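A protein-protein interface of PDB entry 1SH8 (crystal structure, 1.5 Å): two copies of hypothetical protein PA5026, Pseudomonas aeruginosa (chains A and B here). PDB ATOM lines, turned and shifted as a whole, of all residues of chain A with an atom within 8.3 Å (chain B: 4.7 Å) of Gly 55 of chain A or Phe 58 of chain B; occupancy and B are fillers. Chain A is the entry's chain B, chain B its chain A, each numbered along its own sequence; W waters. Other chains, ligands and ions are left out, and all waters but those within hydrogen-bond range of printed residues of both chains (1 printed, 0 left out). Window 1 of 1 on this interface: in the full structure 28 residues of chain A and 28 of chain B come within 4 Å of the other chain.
OH of Tyr 53 of chain A sits at hydrogen-bond distance from OE1 of Glu 62 of chain B (2.6 Å). The backbone carbonyl oxygen of Met 85 of chain B is in hydrogen-bond range of the backbone NH of Leu 87 of chain A (2.8 Å). O of Met 85 of chain A sits at hydrogen-bond distance from N of Leu 87 of chain B (2.8 Å).
The backbone carbonyl oxygen (O) of Gly 55 of chain B lies within hydrogen-bond range of the side-chain hydroxyl (OG1) of Thr 59 of chain B. SD of Met 40 of chain A sits close to OD1 of Asn 45 of chain A (3.6 Å). O of Ser 24 of chain A lies close to OD1 of Asn 45 of chain A, 3.0 Å away. The backbone carbonyl oxygen (O) of Asn 45 of chain A is in hydrogen-bond range of the backbone NH (N) of Tyr 53 of chain A, 2.8 Å away. The side-chain hydroxyl of Thr 59 of chain A sits at hydrogen-bond distance from the backbone carbonyl oxygen of Gly 55 of chain A, 2.9 Å away.
Among the printed residues, merely in contact across the chains: Phe 58 of chain A with Phe 58 of chain B, Thr 86 of chain A with Met 85 of chain B, Tyr 53 of chain A with Phe 20 of chain B, Asn 45 of chain A with Phe 20 of chain B, Phe 20 of chain A with Phe 20 of chain B, Phe 58 of chain A with Ala 54 of chain B, Phe 20 of chain A with Gly 55 of chain B, Gly 55 of chain A with Phe 20 of chain B, Ala 54 of chain A with Phe 58 of chain B, Phe 20 of chain A with Ala 56 of chain B, Ala 56 of chain A with Phe 20 of chain B, Tyr 53 of chain A with Thr 59 of chain B, Phe 58 of chain A with Gly 55 of chain B, Gly 55 of chain A with Phe 58 of chain B, Met 85 of chain A with Met 85 of chain B, Thr 59 of chain A with Phe 20 of chain B, Glu 62 of chain A with Ala 54 of chain B, Phe 20 of chain A with Thr 59 of chain B and Phe 89 of chain A with Phe 58 of chain B.
Of chain B, only Phe 20 and Phe 58 come within 4 Å of Gly 55 of chain A. Of the printed residues of chain A, Phe 58 of chain B touches Ala 54, Gly 55, Phe 58 and Phe 89. Printed residues of chain B within 4 Å of Asn 45 of chain A: Phe 20 (3.4 Å). Printed residues of chain B within 4 Å of Ala 56 of chain A: Phe 20. Leu 60 of chain A touches none of the printed residues of chain B. Leu 57 of chain B touches none of the printed residues of chain A. The nearest residue of chain B that does not touch Gly 55 of chain A is Thr 59 of chain B (4.1 Å). The nearest printed residue of chain A that does not touch Phe 58 of chain B is Leu 87 of chain A (5.0 Å). The nearest printed residue of chain B that does not touch Glu 62 of chain A is Gly 55 of chain B (5.3 Å).
Of the 12 printed residues of chain B, 9 touch a printed residue of chain A. Printed residues of chain B that touch a printed residue of chain A: Phe 20, Ala 54, Gly 55, Ala 56, Phe 58, Thr 59, Glu 62, Met 85 and Leu 87. Of the 21 printed residues of chain A, 13 touch a printed residue of chain B. Among the printed residues, no Asp or Glu carboxylate lies within 4 Å of a Lys or Arg side-chain nitrogen of the other chain.
Phe 20 of chain B touches its own counterpart, Phe 20 of chain A. Phe 20 of chain A touches Gly 55 of chain B, and with the chains exchanged Gly 55 of chain A touches Phe 20 of chain B. Phe 20 of chain A touches Thr 59 of chain B, and with the chains exchanged Thr 59 of chain A touches Phe 20 of chain B. Gly 55 of chain A touches Phe 58 of chain B, and with the chains exchanged Phe 58 of chain A touches Gly 55 of chain B. Of the 22 pairs that touch across the chains among the printed residues, 15 have their exchanged pair printed and touching as well.
Water W1 lies within hydrogen-bond range of the backbone carbonyl oxygen of Met 85 of chain B and the backbone carbonyl oxygen of Met 85 of chain A.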
ATOM      1  N   PHE A  20      36.817  17.590  -7.207  1.00  0.00           N
ATOM      2  CA  PHE A  20      35.471  17.073  -7.455  1.00  0.00           C
ATOM      3  C   PHE A  20      34.957  17.609  -8.794  1.00  0.00           C
ATOM      4  O   PHE A  20      34.360  16.877  -9.588  1.00  0.00           O
ATOM      5  CB  PHE A  20      34.545  17.511  -6.317  1.00  0.00           C
ATOM      6  CG  PHE A  20      33.136  16.982  -6.420  1.00  0.00           C
ATOM      7  CD1 PHE A  20      32.725  15.903  -5.639  1.00  0.00           C
ATOM      8  CD2 PHE A  20      32.207  17.597  -7.259  1.00  0.00           C
ATOM      9  CE1 PHE A  20      31.401  15.443  -5.685  1.00  0.00           C
ATOM     10  CE2 PHE A  20      30.884  17.149  -7.315  1.00  0.00           C
ATOM     11  CZ  PHE A  20      30.482  16.069  -6.523  1.00  0.00           C
ATOM     12  N   SER A  24      34.722  15.845 -13.089  1.00  0.00           N
ATOM     13  CA  SER A  24      33.482  15.836 -13.862  1.00  0.00           C
ATOM     14  C   SER A  24      33.691  16.281 -15.311  1.00  0.00           C
ATOM     15  O   SER A  24      32.832  16.046 -16.166  1.00  0.00           O
ATOM     16  CB  SER A  24      32.430  16.732 -13.200  1.00  0.00           C
ATOM     17  OG  SER A  24      32.719  18.105 -13.391  1.00  0.00           O
ATOM     18  N   MET A  40      28.905  21.258 -18.981  1.00  0.00           N
ATOM     19  CA  MET A  40      29.185  20.009 -18.280  1.00  0.00           C
ATOM     20  C   MET A  40      28.988  18.927 -19.336  1.00  0.00           C
ATOM     21  O   MET A  40      27.902  18.788 -19.897  1.00  0.00           O
ATOM     22  CB  MET A  40      28.216  19.773 -17.113  1.00  0.00           C
ATOM     23  CG  MET A  40      28.506  18.487 -16.315  1.00  0.00           C
ATOM     24  SD  MET A  40      30.072  18.473 -15.372  1.00  0.00           S
ATOM     25  CE  MET A  40      29.580  19.503 -13.962  1.00  0.00           C
ATOM     26  N   ASN A  45      29.135  11.514 -16.873  1.00  0.00           N
ATOM     27  CA  ASN A  45      28.228  12.083 -15.876  1.00  0.00           C
ATOM     28  C   ASN A  45      26.808  11.528 -15.928  1.00  0.00           C
ATOM     29  O   ASN A  45      25.889  12.095 -15.340  1.00  0.00           O
ATOM     30  CB  ASN A  45      28.206  13.602 -16.043  1.00  0.00           C
ATOM     31  CG  ASN A  45      29.553  14.224 -15.750  1.00  0.00           C
ATOM     32  OD1 ASN A  45      30.076  15.024 -16.531  1.00  0.00           O
ATOM     33  ND2 ASN A  45      30.127  13.853 -14.620  1.00  0.00           N
ATOM     34  N   ASN A  47      23.546   9.051 -15.296  1.00  0.00           N
ATOM     35  CA  ASN A  47      22.982   8.417 -14.119  1.00  0.00           C
ATOM     36  C   ASN A  47      22.561   6.987 -14.451  1.00  0.00           C
ATOM     37  O   ASN A  47      23.091   6.372 -15.375  1.00  0.00           O
ATOM     38  CB  ASN A  47      21.780   9.211 -13.592  1.00  0.00           C
ATOM     39  CG  ASN A  47      20.671   9.373 -14.626  1.00  0.00           C
ATOM     40  OD1 ASN A  47      20.597   8.637 -15.610  1.00  0.00           O
ATOM     41  ND2 ASN A  47      19.792  10.340 -14.392  1.00  0.00           N
ATOM     42  N   MET A  52      21.953  12.923 -17.559  1.00  0.00           N
ATOM     43  CA  MET A  52      22.911  13.474 -16.602  1.00  0.00           C
ATOM     44  C   MET A  52      22.461  13.311 -15.153  1.00  0.00           C
ATOM     45  O   MET A  52      21.311  13.594 -14.809  1.00  0.00           O
ATOM     46  CB  MET A  52      23.184  14.957 -16.899  1.00  0.00           C
ATOM     47  CG  MET A  52      24.308  15.567 -16.058  1.00  0.00           C
ATOM     48  SD  MET A  52      24.838  17.232 -16.599  1.00  0.00           S
ATOM     49  CE  MET A  52      25.785  16.797 -18.091  1.00  0.00           C
ATOM     50  N   TYR A  53      23.376  12.845 -14.310  1.00  0.00           N
ATOM     51  CA  TYR A  53      23.087  12.662 -12.895  1.00  0.00           C
ATOM     52  C   TYR A  53      22.771  14.017 -12.251  1.00  0.00           C
ATOM     53  O   TYR A  53      23.393  15.030 -12.575  1.00  0.00           O
ATOM     54  CB  TYR A  53      24.284  12.002 -12.192  1.00  0.00           C
ATOM     55  CG  TYR A  53      24.119  11.920 -10.691  1.00  0.00           C
ATOM     56  CD1 TYR A  53      22.988  11.323 -10.126  1.00  0.00           C
ATOM     57  CD2 TYR A  53      25.053  12.502  -9.837  1.00  0.00           C
ATOM     58  CE1 TYR A  53      22.785  11.322  -8.747  1.00  0.00           C
ATOM     59  CE2 TYR A  53      24.863  12.504  -8.457  1.00  0.00           C
ATOM     60  CZ  TYR A  53      23.721  11.918  -7.919  1.00  0.00           C
ATOM     61  OH  TYR A  53      23.495  11.984  -6.564  1.00  0.00           O
ATOM     62  N   ALA A  54      21.797  14.028 -11.348  1.00  0.00           N
ATOM     63  CA  ALA A  54      21.389  15.252 -10.666  1.00  0.00           C
ATOM     64  C   ALA A  54      22.562  16.005 -10.032  1.00  0.00           C
ATOM     65  O   ALA A  54      22.584  17.238 -10.033  1.00  0.00           O
ATOM     66  CB  ALA A  54      20.336  14.926  -9.599  1.00  0.00           C
ATOM     67  N   GLY A  55      23.527  15.268  -9.487  1.00  0.00           N
ATOM     68  CA  GLY A  55      24.671  15.904  -8.856  1.00  0.00           C
ATOM     69  C   GLY A  55      25.552  16.668  -9.835  1.00  0.00           C
ATOM     70  O   GLY A  55      26.186  17.654  -9.460  1.00  0.00           O
ATOM     71  N   ALA A  56      25.614  16.202 -11.081  1.00  0.00           N
ATOM     72  CA  ALA A  56      26.415  16.870 -12.103  1.00  0.00           C
ATOM     73  C   ALA A  56      25.686  18.146 -12.520  1.00  0.00           C
ATOM     74  O   ALA A  56      26.311  19.189 -12.739  1.00  0.00           O
ATOM     75  CB  ALA A  56      26.617  15.948 -13.307  1.00  0.00           C
ATOM     76  N   LEU A  57      24.361  18.060 -12.631  1.00  0.00           N
ATOM     77  CA  LEU A  57      23.564  19.230 -12.990  1.00  0.00           C
ATOM     78  C   LEU A  57      23.696  20.266 -11.872  1.00  0.00           C
ATOM     79  O   LEU A  57      23.814  21.464 -12.138  1.00  0.00           O
ATOM     80  CB  LEU A  57      22.095  18.836 -13.188  1.00  0.00           C
ATOM     81  CG  LEU A  57      21.788  18.046 -14.472  1.00  0.00           C
ATOM     82  CD1 LEU A  57      20.411  17.409 -14.375  1.00  0.00           C
ATOM     83  CD2 LEU A  57      21.862  18.986 -15.687  1.00  0.00           C
ATOM     84  N   PHE A  58      23.692  19.805 -10.620  1.00  0.00           N
ATOM     85  CA  PHE A  58      23.837  20.720  -9.490  1.00  0.00           C
ATOM     86  C   PHE A  58      25.175  21.443  -9.562  1.00  0.00           C
ATOM     87  O   PHE A  58      25.250  22.656  -9.371  1.00  0.00           O
ATOM     88  CB  PHE A  58      23.768  19.976  -8.157  1.00  0.00           C
ATOM     89  CG  PHE A  58      24.084  20.846  -6.975  1.00  0.00           C
ATOM     90  CD1 PHE A  58      23.078  21.579  -6.338  1.00  0.00           C
ATOM     91  CD2 PHE A  58      25.397  20.983  -6.534  1.00  0.00           C
ATOM     92  CE1 PHE A  58      23.384  22.440  -5.274  1.00  0.00           C
ATOM     93  CE2 PHE A  58      25.715  21.841  -5.475  1.00  0.00           C
ATOM     94  CZ  PHE A  58      24.706  22.569  -4.846  1.00  0.00           C
ATOM     95  N   THR A  59      26.235  20.684  -9.832  1.00  0.00           N
ATOM     96  CA  THR A  59      27.575  21.246  -9.914  1.00  0.00           C
ATOM     97  C   THR A  59      27.643  22.315 -11.007  1.00  0.00           C
ATOM     98  O   THR A  59      28.244  23.372 -10.816  1.00  0.00           O
ATOM     99  CB  THR A  59      28.610  20.128 -10.163  1.00  0.00           C
ATOM    100  OG1 THR A  59      28.582  19.215  -9.054  1.00  0.00           O
ATOM    101  CG2 THR A  59      30.017  20.697 -10.297  1.00  0.00           C
ATOM    102  N   LEU A  60      27.011  22.037 -12.142  1.00  0.00           N
ATOM    103  CA  LEU A  60      26.976  22.989 -13.249  1.00  0.00           C
ATOM    104  C   LEU A  60      26.277  24.278 -12.826  1.00  0.00           C
ATOM    105  O   LEU A  60      26.696  25.375 -13.202  1.00  0.00           O
ATOM    106  CB  LEU A  60      26.234  22.384 -14.446  1.00  0.00           C
ATOM    107  CG  LEU A  60      26.052  23.280 -15.678  1.00  0.00           C
ATOM    108  CD1 LEU A  60      27.417  23.715 -16.222  1.00  0.00           C
ATOM    109  CD2 LEU A  60      25.254  22.518 -16.735  1.00  0.00           C
ATOM    110  N   ALA A  61      25.212  24.143 -12.039  1.00  0.00           N
ATOM    111  CA  ALA A  61      24.444  25.295 -11.573  1.00  0.00           C
ATOM    112  C   ALA A  61      25.130  26.055 -10.438  1.00  0.00           C
ATOM    113  O   ALA A  61      24.951  27.262 -10.294  1.00  0.00           O
ATOM    114  CB  ALA A  61      23.058  24.842 -11.122  1.00  0.00           C
ATOM    115  N   GLU A  62      25.920  25.345  -9.641  1.00  0.00           N
ATOM    116  CA  GLU A  62      26.608  25.938  -8.490  1.00  0.00           C
ATOM    117  C   GLU A  62      27.841  26.770  -8.845  1.00  0.00           C
ATOM    118  O   GLU A  62      28.038  27.861  -8.301  1.00  0.00           O
ATOM    119  CB  GLU A  62      27.006  24.815  -7.518  1.00  0.00           C
ATOM    120  CG  GLU A  62      27.542  25.241  -6.150  1.00  0.00           C
ATOM    121  CD  GLU A  62      28.995  25.710  -6.156  1.00  0.00           C
ATOM    122  OE1 GLU A  62      29.774  25.329  -7.062  1.00  0.00           O
ATOM    123  OE2 GLU A  62      29.365  26.452  -5.223  1.00  0.00           O
ATOM    124  N   MET A  85      20.407  26.495  -2.162  1.00  0.00           N
ATOM    125  CA  MET A  85      20.190  26.348  -3.590  1.00  0.00           C
ATOM    126  C   MET A  85      19.043  25.383  -3.830  1.00  0.00           C
ATOM    127  O   MET A  85      18.910  24.378  -3.133  1.00  0.00           O
ATOM    128  CB  MET A  85      21.447  25.815  -4.272  1.00  0.00           C
ATOM    129  CG  MET A  85      22.564  26.841  -4.400  1.00  0.00           C
ATOM    130  SD  MET A  85      23.983  26.224  -5.349  1.00  0.00           S
ATOM    131  CE  MET A  85      23.194  25.900  -6.972  1.00  0.00           C
ATOM    132  N   THR A  86      18.209  25.707  -4.809  1.00  0.00           N
ATOM    133  CA  THR A  86      17.085  24.861  -5.168  1.00  0.00           C
ATOM    134  C   THR A  86      17.216  24.504  -6.632  1.00  0.00           C
ATOM    135  O   THR A  86      17.479  25.368  -7.468  1.00  0.00           O
ATOM    136  CB  THR A  86      15.733  25.573  -4.969  1.00  0.00           C
ATOM    137  OG1 THR A  86      15.519  25.818  -3.574  1.00  0.00           O
ATOM    138  CG2 THR A  86      14.599  24.709  -5.503  1.00  0.00           C
ATOM    139  N   LEU A  87      17.042  23.222  -6.934  1.00  0.00           N
ATOM    140  CA  LEU A  87      17.117  22.731  -8.301  1.00  0.00           C
ATOM    141  C   LEU A  87      15.784  22.115  -8.682  1.00  0.00           C
ATOM    142  O   LEU A  87      15.156  21.423  -7.882  1.00  0.00           O
ATOM    143  CB  LEU A  87      18.205  21.661  -8.440  1.00  0.00           C
ATOM    144  CG  LEU A  87      19.608  22.061  -8.904  1.00  0.00           C
ATOM    145  CD1 LEU A  87      19.557  22.457 -10.374  1.00  0.00           C
ATOM    146  CD2 LEU A  87      20.142  23.196  -8.041  1.00  0.00           C
ATOM    147  N   ARG A  88      15.349  22.391  -9.901  1.00  0.00           N
ATOM    148  CA  ARG A  88      14.120  21.820 -10.410  1.00  0.00           C
ATOM    149  C   ARG A  88      14.553  21.073 -11.663  1.00  0.00           C
ATOM    150  O   ARG A  88      15.117  21.666 -12.585  1.00  0.00           O
ATOM    151  CB  ARG A  88      13.116  22.918 -10.746  1.00  0.00           C
ATOM    152  CG  ARG A  88      11.764  22.408 -11.186  1.00  0.00           C
ATOM    153  CD  ARG A  88      10.730  23.524 -11.079  1.00  0.00           C
ATOM    154  NE  ARG A  88       9.419  23.118 -11.584  1.00  0.00           N
ATOM    155  CZ  ARG A  88       9.130  22.948 -12.872  1.00  0.00           C
ATOM    156  NH1 ARG A  88      10.058  23.151 -13.798  1.00  0.00           N
ATOM    157  NH2 ARG A  88       7.907  22.577 -13.233  1.00  0.00           N
ATOM    158  N   PHE A  89      14.321  19.764 -11.673  1.00  0.00           N
ATOM    159  CA  PHE A  89      14.696  18.918 -12.799  1.00  0.00           C
ATOM    160  C   PHE A  89      13.469  18.749 -13.685  1.00  0.00           C
ATOM    161  O   PHE A  89      12.568  17.963 -13.390  1.00  0.00           O
ATOM    162  CB  PHE A  89      15.217  17.584 -12.258  1.00  0.00           C
ATOM    163  CG  PHE A  89      16.377  17.748 -11.313  1.00  0.00           C
ATOM    164  CD1 PHE A  89      17.653  18.024 -11.799  1.00  0.00           C
ATOM    165  CD2 PHE A  89      16.184  17.699  -9.936  1.00  0.00           C
ATOM    166  CE1 PHE A  89      18.717  18.251 -10.928  1.00  0.00           C
ATOM    167  CE2 PHE A  89      17.241  17.924  -9.055  1.00  0.00           C
ATOM    168  CZ  PHE A  89      18.511  18.201  -9.551  1.00  0.00           C
ATOM    169  N   PHE B  20      29.718   9.162 -11.483  1.00  0.00           N
ATOM    170  CA  PHE B  20      29.900  10.450 -10.821  1.00  0.00           C
ATOM    171  C   PHE B  20      29.956  10.216  -9.312  1.00  0.00           C
ATOM    172  O   PHE B  20      30.780  10.805  -8.607  1.00  0.00           O
ATOM    173  CB  PHE B  20      28.720  11.362 -11.175  1.00  0.00           C
ATOM    174  CG  PHE B  20      28.800  12.748 -10.583  1.00  0.00           C
ATOM    175  CD1 PHE B  20      29.297  13.813 -11.334  1.00  0.00           C
ATOM    176  CD2 PHE B  20      28.341  12.995  -9.290  1.00  0.00           C
ATOM    177  CE1 PHE B  20      29.329  15.112 -10.807  1.00  0.00           C
ATOM    178  CE2 PHE B  20      28.370  14.282  -8.756  1.00  0.00           C
ATOM    179  CZ  PHE B  20      28.863  15.343  -9.515  1.00  0.00           C
ATOM    180  N   ALA B  54      30.254  22.049  -2.192  1.00  0.00           N
ATOM    181  CA  ALA B  54      28.790  22.006  -2.245  1.00  0.00           C
ATOM    182  C   ALA B  54      28.230  20.848  -3.068  1.00  0.00           C
ATOM    183  O   ALA B  54      27.207  20.270  -2.704  1.00  0.00           O
ATOM    184  CB  ALA B  54      28.254  23.327  -2.786  1.00  0.00           C
ATOM    185  N   GLY B  55      28.893  20.527  -4.179  1.00  0.00           N
ATOM    186  CA  GLY B  55      28.449  19.444  -5.045  1.00  0.00           C
ATOM    187  C   GLY B  55      28.523  18.085  -4.371  1.00  0.00           C
ATOM    188  O   GLY B  55      27.707  17.197  -4.651  1.00  0.00           O
ATOM    189  N   ALA B  56      29.504  17.916  -3.488  1.00  0.00           N
ATOM    190  CA  ALA B  56      29.659  16.663  -2.758  1.00  0.00           C
ATOM    191  C   ALA B  56      28.537  16.580  -1.721  1.00  0.00           C
ATOM    192  O   ALA B  56      27.958  15.510  -1.504  1.00  0.00           O
ATOM    193  CB  ALA B  56      31.019  16.613  -2.084  1.00  0.00           C
ATOM    194  N   LEU B  57      28.236  17.708  -1.072  1.00  0.00           N
ATOM    195  CA  LEU B  57      27.156  17.746  -0.086  1.00  0.00           C
ATOM    196  C   LEU B  57      25.839  17.415  -0.783  1.00  0.00           C
ATOM    197  O   LEU B  57      25.029  16.644  -0.265  1.00  0.00           O
ATOM    198  CB  LEU B  57      27.081  19.129   0.570  1.00  0.00           C
ATOM    199  CG  LEU B  57      28.189  19.427   1.590  1.00  0.00           C
ATOM    200  CD1 LEU B  57      28.221  20.914   1.929  1.00  0.00           C
ATOM    201  CD2 LEU B  57      27.947  18.587   2.848  1.00  0.00           C
ATOM    202  N   PHE B  58      25.634  17.981  -1.967  1.00  0.00           N
ATOM    203  CA  PHE B  58      24.402  17.714  -2.710  1.00  0.00           C
ATOM    204  C   PHE B  58      24.271  16.232  -3.039  1.00  0.00           C
ATOM    205  O   PHE B  58      23.208  15.637  -2.873  1.00  0.00           O
ATOM    206  CB  PHE B  58      24.366  18.501  -4.021  1.00  0.00           C
ATOM    207  CG  PHE B  58      23.131  18.235  -4.843  1.00  0.00           C
ATOM    208  CD1 PHE B  58      21.979  19.002  -4.674  1.00  0.00           C
ATOM    209  CD2 PHE B  58      23.107  17.186  -5.760  1.00  0.00           C
ATOM    210  CE1 PHE B  58      20.816  18.723  -5.414  1.00  0.00           C
ATOM    211  CE2 PHE B  58      21.954  16.898  -6.499  1.00  0.00           C
ATOM    212  CZ  PHE B  58      20.809  17.668  -6.325  1.00  0.00           C
ATOM    213  N   THR B  59      25.358  15.639  -3.523  1.00  0.00           N
ATOM    214  CA  THR B  59      25.340  14.232  -3.889  1.00  0.00           C
ATOM    215  C   THR B  59      24.990  13.360  -2.684  1.00  0.00           C
ATOM    216  O   THR B  59      24.179  12.437  -2.792  1.00  0.00           O
ATOM    217  CB  THR B  59      26.695  13.817  -4.495  1.00  0.00           C
ATOM    218  OG1 THR B  59      26.917  14.571  -5.693  1.00  0.00           O
ATOM    219  CG2 THR B  59      26.705  12.338  -4.845  1.00  0.00           C
ATOM    220  N   LEU B  60      25.583  13.664  -1.534  1.00  0.00           N
ATOM    221  CA  LEU B  60      25.304  12.900  -0.322  1.00  0.00           C
ATOM    222  C   LEU B  60      23.837  13.024   0.086  1.00  0.00           C
ATOM    223  O   LEU B  60      23.206  12.040   0.466  1.00  0.00           O
ATOM    224  CB  LEU B  60      26.184  13.392   0.831  1.00  0.00           C
ATOM    225  CG  LEU B  60      25.912  12.711   2.179  1.00  0.00           C
ATOM    226  CD1 LEU B  60      26.208  11.218   2.062  1.00  0.00           C
ATOM    227  CD2 LEU B  60      26.770  13.345   3.261  1.00  0.00           C
ATOM    228  N   ALA B  61      23.303  14.242   0.003  1.00  0.00           N
ATOM    229  CA  ALA B  61      21.915  14.504   0.384  1.00  0.00           C
ATOM    230  C   ALA B  61      20.891  13.957  -0.606  1.00  0.00           C
ATOM    231  O   ALA B  61      19.784  13.588  -0.220  1.00  0.00           O
ATOM    232  CB  ALA B  61      21.706  16.005   0.558  1.00  0.00           C
ATOM    233  N   GLU B  62      21.268  13.897  -1.879  1.00  0.00           N
ATOM    234  CA  GLU B  62      20.373  13.438  -2.940  1.00  0.00           C
ATOM    235  C   GLU B  62      20.272  11.916  -3.109  1.00  0.00           C
ATOM    236  O   GLU B  62      19.185  11.379  -3.362  1.00  0.00           O
ATOM    237  CB  GLU B  62      20.824  14.070  -4.270  1.00  0.00           C
ATOM    238  CG  GLU B  62      19.876  13.914  -5.464  1.00  0.00           C
ATOM    239  CD  GLU B  62      19.860  12.518  -6.087  1.00  0.00           C
ATOM    240  OE1 GLU B  62      20.905  11.828  -6.096  1.00  0.00           O
ATOM    241  OE2 GLU B  62      18.788  12.121  -6.598  1.00  0.00           O
ATOM    242  N   MET B  85      14.752  19.711  -5.526  1.00  0.00           N
ATOM    243  CA  MET B  85      15.445  19.591  -4.259  1.00  0.00           C
ATOM    244  C   MET B  85      16.036  20.916  -3.820  1.00  0.00           C
ATOM    245  O   MET B  85      16.553  21.684  -4.636  1.00  0.00           O
ATOM    246  CB  MET B  85      16.556  18.542  -4.391  1.00  0.00           C
ATOM    247  CG  MET B  85      17.366  18.272  -3.127  1.00  0.00           C
ATOM    248  SD  MET B  85      18.503  16.848  -3.315  1.00  0.00           S
ATOM    249  CE  MET B  85      17.499  15.681  -3.971  1.00  0.00           C
ATOM    250  N   LEU B  87      18.708  22.535  -0.970  1.00  0.00           N
ATOM    251  CA  LEU B  87      19.814  22.195  -0.071  1.00  0.00           C
ATOM    252  C   LEU B  87      20.216  23.469   0.665  1.00  0.00           C
ATOM    253  O   LEU B  87      20.601  24.451   0.036  1.00  0.00           O
ATOM    254  CB  LEU B  87      21.010  21.655  -0.864  1.00  0.00           C
ATOM    255  CG  LEU B  87      22.248  21.246  -0.051  1.00  0.00           C
ATOM    256  CD1 LEU B  87      21.886  20.142   0.944  1.00  0.00           C
ATOM    257  CD2 LEU B  87      23.349  20.771  -0.993  1.00  0.00           C
HETATM  258  O   HOH W   1      19.596  21.584  -4.342  1.00  0.00           O
